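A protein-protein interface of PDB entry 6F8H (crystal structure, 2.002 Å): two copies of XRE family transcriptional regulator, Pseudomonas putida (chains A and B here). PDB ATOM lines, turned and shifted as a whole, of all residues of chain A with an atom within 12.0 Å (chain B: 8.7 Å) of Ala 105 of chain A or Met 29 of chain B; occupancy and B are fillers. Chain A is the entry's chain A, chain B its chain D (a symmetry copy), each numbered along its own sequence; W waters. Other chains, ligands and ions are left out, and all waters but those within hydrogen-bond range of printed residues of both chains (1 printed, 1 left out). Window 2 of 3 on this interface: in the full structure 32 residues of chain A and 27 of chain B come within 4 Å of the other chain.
Of the printed residues of chain B, Val 100 of chain A touches Ala 39 and Cys 68.
Of the printed residues of chain B, Gln 101 of chain A touches Ala 39 and Cys 68.
Of the printed residues of chain B, Leu 103 of chain A touches Met 29, Phe 31 and Cys 68.
Of chain B, only Met 29 (3.8 Å) comes within 4 Å of Ala 105 of chain A.
No residue of chain A comes within 4 Å of Phe 25 of chain B.
No residue of chain A comes within 4 Å of Glu 28 of chain B.
Met 29 of chain B touches three residues of chain A.
Gly 30 of chain B touches none of the printed residues of chain A.
Of chain A, only Leu 103 (3.5 Å) comes within 4 Å of Phe 31 of chain B.
No residue of chain A comes within 4 Å of Leu 69 of chain B.
Of the printed residues of chain A, Asp 70 of chain B touches Arg 102 (2.9 Å).
Hydrophobic or aromatic side chains of chain B that line the printed part of chain A: Met 29, Phe 31 and Ala 39.
Of the 6 printed residues of chain A, 6 touch a printed residue of chain B.
Hydrophobic or aromatic side chains of chain A within 4 Å of the printed part of chain B: Val 100 and Leu 103.
Among the printed residues, 11 pairs touch across the chains.
Among the printed residues, Asp or Glu carboxylates within 4 Å of a Lys or Arg side-chain nitrogen of the other chain: Arg 102 of chain A with Asp 70 of chain B (2.9 Å).
N of Gln 101 of chain A lies within hydrogen-bond range of O of Ala 39 of chain B.
The side-chain sulfur (SG) of Cys 68 of chain B is in hydrogen-bond range of the backbone carbonyl oxygen (O) of Gln 101 of chain A (3.6 Å).
The side-chain carboxylate of Asp 70 of chain B lies within salt-bridge range of the guanidinium group of Arg 102 of chain A (2.9 Å).
N of Leu 103 of chain A is in hydrogen-bond range of O of Cys 68 of chain B, at 2.8 Å.
Among the printed residues, pairs that only touch across the chains: Leu 103 of chain A with Met 29 of chain B (3.0 Å), Arg 102 of chain A with Cys 68 of chain B (3.3 Å), Val 100 of chain A with Ala 39 of chain B (3.4 Å), Val 104 of chain A with Met 29 of chain B (3.5 Å), Leu 103 of chain A with Phe 31 of chain B (3.5 Å), Ala 105 of chain A with Met 29 of chain B (3.8 Å) and Val 100 of chain A with Cys 68 of chain B (3.9 Å).
No position is printed for both chains.
Of the 11 pairs that touch across the chains among the printed residues, none has its exchanged pair printed and touching as well.
Water W1 bridges OD1 of Asp 70 of chain B and NE of Arg 102 of chain A.
The side-chain amide nitrogen (NE2) of Gln 26 of chain B is in hydrogen-bond range of the backbone carbonyl oxygen (O) of Phe 31 of chain B (3.3 Å).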
ATOM      1  N   VAL A 100     -15.738  31.094  32.012  1.00  0.00           N
ATOM      2  CA  VAL A 100     -14.888  30.350  31.080  1.00  0.00           C
ATOM      3  C   VAL A 100     -13.537  30.018  31.701  1.00  0.00           C
ATOM      4  O   VAL A 100     -12.907  30.865  32.325  1.00  0.00           O
ATOM      5  CB  VAL A 100     -14.652  31.124  29.744  1.00  0.00           C
ATOM      6  CG1 VAL A 100     -13.634  30.392  28.869  1.00  0.00           C
ATOM      7  CG2 VAL A 100     -15.965  31.312  28.984  1.00  0.00           C
ATOM      8  N   GLN A 101     -13.110  28.772  31.523  1.00  0.00           N
ATOM      9  CA  GLN A 101     -11.794  28.315  31.954  1.00  0.00           C
ATOM     10  C   GLN A 101     -10.862  28.184  30.743  1.00  0.00           C
ATOM     11  O   GLN A 101     -11.294  27.718  29.692  1.00  0.00           O
ATOM     12  CB  GLN A 101     -11.916  26.968  32.670  1.00  0.00           C
ATOM     13  CG  GLN A 101     -12.788  27.000  33.936  1.00  0.00           C
ATOM     14  CD  GLN A 101     -12.105  27.703  35.107  1.00  0.00           C
ATOM     15  OE1 GLN A 101     -12.182  28.929  35.250  1.00  0.00           O
ATOM     16  NE2 GLN A 101     -11.438  26.923  35.953  1.00  0.00           N
ATOM     17  N   ARG A 102      -9.591  28.569  30.863  1.00  0.00           N
ATOM     18  CA  ARG A 102      -8.718  28.347  29.719  1.00  0.00           C
ATOM     19  C   ARG A 102      -8.376  26.866  29.648  1.00  0.00           C
ATOM     20  O   ARG A 102      -8.367  26.155  30.649  1.00  0.00           O
ATOM     21  CB  ARG A 102      -7.457  29.232  29.748  1.00  0.00           C
ATOM     22  CG  ARG A 102      -6.721  29.338  31.047  1.00  0.00           C
ATOM     23  CD  ARG A 102      -5.725  30.514  31.011  1.00  0.00           C
ATOM     24  NE  ARG A 102      -4.654  30.322  30.033  1.00  0.00           N
ATOM     25  CZ  ARG A 102      -3.500  29.713  30.301  1.00  0.00           C
ATOM     26  NH1 ARG A 102      -3.276  29.224  31.518  1.00  0.00           N
ATOM     27  NH2 ARG A 102      -2.577  29.582  29.358  1.00  0.00           N
ATOM     28  N   LEU A 103      -8.156  26.401  28.429  1.00  0.00           N
ATOM     29  CA  LEU A 103      -7.820  25.013  28.187  1.00  0.00           C
ATOM     30  C   LEU A 103      -6.440  24.953  27.552  1.00  0.00           C
ATOM     31  O   LEU A 103      -6.246  25.457  26.445  1.00  0.00           O
ATOM     32  CB  LEU A 103      -8.862  24.360  27.281  1.00  0.00           C
ATOM     33  CG  LEU A 103      -8.951  22.840  27.340  1.00  0.00           C
ATOM     34  CD1 LEU A 103      -9.447  22.392  28.717  1.00  0.00           C
ATOM     35  CD2 LEU A 103      -9.862  22.323  26.244  1.00  0.00           C
ATOM     36  N   VAL A 104      -5.475  24.362  28.245  1.00  0.00           N
ATOM     37  CA  VAL A 104      -4.127  24.225  27.690  1.00  0.00           C
ATOM     38  C   VAL A 104      -3.803  22.761  27.420  1.00  0.00           C
ATOM     39  O   VAL A 104      -2.769  22.440  26.849  1.00  0.00           O
ATOM     40  CB  VAL A 104      -3.068  24.816  28.623  1.00  0.00           C
ATOM     41  CG1 VAL A 104      -3.379  26.290  28.919  1.00  0.00           C
ATOM     42  CG2 VAL A 104      -2.994  24.008  29.912  1.00  0.00           C
ATOM     43  N   ALA A 105      -4.710  21.876  27.831  1.00  0.00           N
ATOM     44  CA  ALA A 105      -4.555  20.442  27.601  1.00  0.00           C
ATOM     45  C   ALA A 105      -5.875  19.701  27.835  1.00  0.00           C
ATOM     46  O   ALA A 105      -6.972  20.226  27.606  1.00  0.00           O
ATOM     47  CB  ALA A 105      -3.455  19.867  28.500  1.00  0.00           C
ATOM     48  OXT ALA A 105      -5.878  18.544  28.261  1.00  0.00           O
ATOM     49  N   LEU B  21     -10.529  25.668  14.306  1.00  0.00           N
ATOM     50  CA  LEU B  21     -10.712  25.181  15.676  1.00  0.00           C
ATOM     51  C   LEU B  21     -10.405  23.678  15.762  1.00  0.00           C
ATOM     52  O   LEU B  21      -9.705  23.221  16.660  1.00  0.00           O
ATOM     53  CB  LEU B  21     -12.141  25.460  16.154  1.00  0.00           C
ATOM     54  CG  LEU B  21     -12.463  25.028  17.583  1.00  0.00           C
ATOM     55  CD1 LEU B  21     -11.595  25.776  18.588  1.00  0.00           C
ATOM     56  CD2 LEU B  21     -13.952  25.238  17.889  1.00  0.00           C
ATOM     57  N   ARG B  22     -10.933  22.926  14.806  1.00  0.00           N
ATOM     58  CA  ARG B  22     -10.743  21.483  14.758  1.00  0.00           C
ATOM     59  C   ARG B  22      -9.288  21.085  14.454  1.00  0.00           C
ATOM     60  O   ARG B  22      -8.673  20.338  15.221  1.00  0.00           O
ATOM     61  CB  ARG B  22     -11.697  20.874  13.718  1.00  0.00           C
ATOM     62  CG  ARG B  22     -11.680  19.369  13.639  1.00  0.00           C
ATOM     63  CD  ARG B  22     -12.639  18.860  12.572  1.00  0.00           C
ATOM     64  NE  ARG B  22     -12.150  19.108  11.217  1.00  0.00           N
ATOM     65  CZ  ARG B  22     -12.723  19.938  10.346  1.00  0.00           C
ATOM     66  NH1 ARG B  22     -13.816  20.619  10.683  1.00  0.00           N
ATOM     67  NH2 ARG B  22     -12.200  20.098   9.137  1.00  0.00           N
ATOM     68  N   GLU B  23      -8.730  21.588  13.354  1.00  0.00           N
ATOM     69  CA  GLU B  23      -7.401  21.152  12.924  1.00  0.00           C
ATOM     70  C   GLU B  23      -6.242  21.796  13.707  1.00  0.00           C
ATOM     71  O   GLU B  23      -5.254  21.130  13.990  1.00  0.00           O
ATOM     72  CB  GLU B  23      -7.215  21.424  11.424  1.00  0.00           C
ATOM     73  CG  GLU B  23      -8.330  20.870  10.538  1.00  0.00           C
ATOM     74  CD  GLU B  23      -8.343  19.347  10.440  1.00  0.00           C
ATOM     75  OE1 GLU B  23      -7.445  18.678  11.003  1.00  0.00           O
ATOM     76  OE2 GLU B  23      -9.269  18.819   9.789  1.00  0.00           O
ATOM     77  N   GLU B  24      -6.357  23.073  14.059  1.00  0.00           N
ATOM     78  CA  GLU B  24      -5.251  23.787  14.712  1.00  0.00           C
ATOM     79  C   GLU B  24      -5.284  23.809  16.243  1.00  0.00           C
ATOM     80  O   GLU B  24      -4.267  24.108  16.884  1.00  0.00           O
ATOM     81  CB  GLU B  24      -5.196  25.234  14.246  1.00  0.00           C
ATOM     82  CG  GLU B  24      -4.808  25.446  12.810  1.00  0.00           C
ATOM     83  CD  GLU B  24      -4.609  26.916  12.502  1.00  0.00           C
ATOM     84  OE1 GLU B  24      -4.373  27.706  13.448  1.00  0.00           O
ATOM     85  OE2 GLU B  24      -4.689  27.290  11.316  1.00  0.00           O
ATOM     86  N   PHE B  25      -6.440  23.547  16.841  1.00  0.00           N
ATOM     87  CA  PHE B  25      -6.507  23.547  18.298  1.00  0.00           C
ATOM     88  C   PHE B  25      -6.911  22.187  18.843  1.00  0.00           C
ATOM     89  O   PHE B  25      -6.205  21.625  19.679  1.00  0.00           O
ATOM     90  CB  PHE B  25      -7.463  24.632  18.799  1.00  0.00           C
ATOM     91  CG  PHE B  25      -6.962  26.027  18.556  1.00  0.00           C
ATOM     92  CD1 PHE B  25      -7.182  26.650  17.335  1.00  0.00           C
ATOM     93  CD2 PHE B  25      -6.259  26.713  19.547  1.00  0.00           C
ATOM     94  CE1 PHE B  25      -6.731  27.935  17.105  1.00  0.00           C
ATOM     95  CE2 PHE B  25      -5.796  27.998  19.320  1.00  0.00           C
ATOM     96  CZ  PHE B  25      -6.032  28.612  18.095  1.00  0.00           C
ATOM     97  N   GLN B  26      -8.030  21.646  18.377  1.00  0.00           N
ATOM     98  CA  GLN B  26      -8.478  20.360  18.900  1.00  0.00           C
ATOM     99  C   GLN B  26      -7.476  19.260  18.605  1.00  0.00           C
ATOM    100  O   GLN B  26      -6.998  18.592  19.516  1.00  0.00           O
ATOM    101  CB  GLN B  26      -9.834  19.960  18.341  1.00  0.00           C
ATOM    102  CG  GLN B  26     -10.307  18.642  18.927  1.00  0.00           C
ATOM    103  CD  GLN B  26     -11.615  18.184  18.361  1.00  0.00           C
ATOM    104  OE1 GLN B  26     -11.924  18.430  17.194  1.00  0.00           O
ATOM    105  NE2 GLN B  26     -12.408  17.507  19.186  1.00  0.00           N
ATOM    106  N   LYS B  27      -7.160  19.074  17.331  1.00  0.00           N
ATOM    107  CA  LYS B  27      -6.218  18.034  16.934  1.00  0.00           C
ATOM    108  C   LYS B  27      -4.864  18.226  17.612  1.00  0.00           C
ATOM    109  O   LYS B  27      -4.200  17.255  17.959  1.00  0.00           O
ATOM    110  CB  LYS B  27      -6.058  18.006  15.414  1.00  0.00           C
ATOM    111  CG  LYS B  27      -5.148  16.895  14.918  1.00  0.00           C
ATOM    112  CD  LYS B  27      -4.782  17.075  13.458  1.00  0.00           C
ATOM    113  CE  LYS B  27      -3.666  16.119  13.076  1.00  0.00           C
ATOM    114  NZ  LYS B  27      -2.543  16.218  14.055  1.00  0.00           N
ATOM    115  N   GLU B  28      -4.473  19.476  17.833  1.00  0.00           N
ATOM    116  CA  GLU B  28      -3.192  19.763  18.463  1.00  0.00           C
ATOM    117  C   GLU B  28      -3.165  19.404  19.939  1.00  0.00           C
ATOM    118  O   GLU B  28      -2.273  18.693  20.397  1.00  0.00           O
ATOM    119  CB  GLU B  28      -2.834  21.241  18.310  1.00  0.00           C
ATOM    120  CG  GLU B  28      -1.703  21.494  17.331  1.00  0.00           C
ATOM    121  CD  GLU B  28      -0.673  20.372  17.326  1.00  0.00           C
ATOM    122  OE1 GLU B  28      -0.040  20.119  18.381  1.00  0.00           O
ATOM    123  OE2 GLU B  28      -0.514  19.731  16.264  1.00  0.00           O
ATOM    124  N   MET B  29      -4.139  19.917  20.682  1.00  0.00           N
ATOM    125  CA  MET B  29      -4.183  19.769  22.138  1.00  0.00           C
ATOM    126  C   MET B  29      -4.976  18.548  22.606  1.00  0.00           C
ATOM    127  O   MET B  29      -5.003  18.235  23.797  1.00  0.00           O
ATOM    128  CB  MET B  29      -4.778  21.029  22.761  1.00  0.00           C
ATOM    129  CG  MET B  29      -4.277  22.315  22.130  1.00  0.00           C
ATOM    130  SD  MET B  29      -5.262  23.738  22.630  1.00  0.00           S
ATOM    131  CE  MET B  29      -5.439  23.381  24.378  1.00  0.00           C
ATOM    132  N   GLY B  30      -5.643  17.880  21.673  1.00  0.00           N
ATOM    133  CA  GLY B  30      -6.281  16.602  21.945  1.00  0.00           C
ATOM    134  C   GLY B  30      -7.483  16.596  22.875  1.00  0.00           C
ATOM    135  O   GLY B  30      -7.813  15.556  23.445  1.00  0.00           O
ATOM    136  N   PHE B  31      -8.151  17.736  23.034  1.00  0.00           N
ATOM    137  CA  PHE B  31      -9.343  17.792  23.881  1.00  0.00           C
ATOM    138  C   PHE B  31     -10.572  17.239  23.160  1.00  0.00           C
ATOM    139  O   PHE B  31     -10.648  17.285  21.939  1.00  0.00           O
ATOM    140  CB  PHE B  31      -9.609  19.232  24.362  1.00  0.00           C
ATOM    141  CG  PHE B  31      -9.814  20.237  23.248  1.00  0.00           C
ATOM    142  CD1 PHE B  31     -10.952  20.203  22.446  1.00  0.00           C
ATOM    143  CD2 PHE B  31      -8.888  21.245  23.038  1.00  0.00           C
ATOM    144  CE1 PHE B  31     -11.146  21.135  21.427  1.00  0.00           C
ATOM    145  CE2 PHE B  31      -9.074  22.187  22.023  1.00  0.00           C
ATOM    146  CZ  PHE B  31     -10.207  22.130  21.222  1.00  0.00           C
ATOM    147  N   SER B  32     -11.533  16.719  23.918  1.00  0.00           N
ATOM    148  CA  SER B  32     -12.825  16.330  23.355  1.00  0.00           C
ATOM    149  C   SER B  32     -13.711  17.554  23.141  1.00  0.00           C
ATOM    150  O   SER B  32     -13.516  18.594  23.792  1.00  0.00           O
ATOM    151  CB  SER B  32     -13.557  15.341  24.274  1.00  0.00           C
ATOM    152  OG  SER B  32     -14.096  16.012  25.407  1.00  0.00           O
ATOM    153  N   ALA B  35     -15.129  18.407  26.487  1.00  0.00           N
ATOM    154  CA  ALA B  35     -14.189  19.112  27.350  1.00  0.00           C
ATOM    155  C   ALA B  35     -14.115  20.591  26.972  1.00  0.00           C
ATOM    156  O   ALA B  35     -14.049  21.462  27.847  1.00  0.00           O
ATOM    157  CB  ALA B  35     -12.807  18.472  27.277  1.00  0.00           C
ATOM    158  N   LEU B  36     -14.124  20.874  25.667  1.00  0.00           N
ATOM    159  CA  LEU B  36     -14.141  22.264  25.205  1.00  0.00           C
ATOM    160  C   LEU B  36     -15.426  22.968  25.653  1.00  0.00           C
ATOM    161  O   LEU B  36     -15.386  24.084  26.157  1.00  0.00           O
ATOM    162  CB  LEU B  36     -14.015  22.347  23.678  1.00  0.00           C
ATOM    163  CG  LEU B  36     -14.009  23.777  23.130  1.00  0.00           C
ATOM    164  CD1 LEU B  36     -12.865  24.590  23.745  1.00  0.00           C
ATOM    165  CD2 LEU B  36     -13.944  23.816  21.629  1.00  0.00           C
ATOM    166  N   ALA B  39     -15.300  23.761  29.277  1.00  0.00           N
ATOM    167  CA  ALA B  39     -14.425  24.912  29.521  1.00  0.00           C
ATOM    168  C   ALA B  39     -15.046  26.217  29.022  1.00  0.00           C
ATOM    169  O   ALA B  39     -14.864  27.259  29.646  1.00  0.00           O
ATOM    170  CB  ALA B  39     -13.051  24.703  28.868  1.00  0.00           C
ATOM    171  N   CYS B  68     -10.627  31.051  26.446  1.00  0.00           N
ATOM    172  CA  CYS B  68     -10.338  29.635  26.574  1.00  0.00           C
ATOM    173  C   CYS B  68      -9.043  29.204  25.887  1.00  0.00           C
ATOM    174  O   CYS B  68      -8.299  28.361  26.413  1.00  0.00           O
ATOM    175  CB  CYS B  68     -11.508  28.831  26.019  1.00  0.00           C
ATOM    176  SG  CYS B  68     -11.361  27.048  26.177  1.00  0.00           S
ATOM    177  N   LEU B  69      -8.764  29.771  24.719  1.00  0.00           N
ATOM    178  CA  LEU B  69      -7.645  29.279  23.925  1.00  0.00           C
ATOM    179  C   LEU B  69      -6.485  30.282  23.823  1.00  0.00           C
ATOM    180  O   LEU B  69      -5.533  30.053  23.080  1.00  0.00           O
ATOM    181  CB  LEU B  69      -8.145  28.884  22.528  1.00  0.00           C
ATOM    182  CG  LEU B  69      -9.231  27.800  22.510  1.00  0.00           C
ATOM    183  CD1 LEU B  69      -9.795  27.552  21.112  1.00  0.00           C
ATOM    184  CD2 LEU B  69      -8.736  26.484  23.137  1.00  0.00           C
ATOM    185  N   ASP B  70      -6.570  31.370  24.584  1.00  0.00           N
ATOM    186  CA  ASP B  70      -5.581  32.461  24.560  1.00  0.00           C
ATOM    187  C   ASP B  70      -5.431  33.086  23.180  1.00  0.00           C
ATOM    188  O   ASP B  70      -4.312  33.250  22.675  1.00  0.00           O
ATOM    189  CB  ASP B  70      -4.216  31.975  25.060  1.00  0.00           C
ATOM    190  CG  ASP B  70      -4.203  31.728  26.547  1.00  0.00           C
ATOM    191  OD1 ASP B  70      -4.660  32.617  27.296  1.00  0.00           O
ATOM    192  OD2 ASP B  70      -3.751  30.645  26.967  1.00  0.00           O
HETATM  193  O   HOH W   1      -2.740  33.208  29.904  1.00  0.00           O
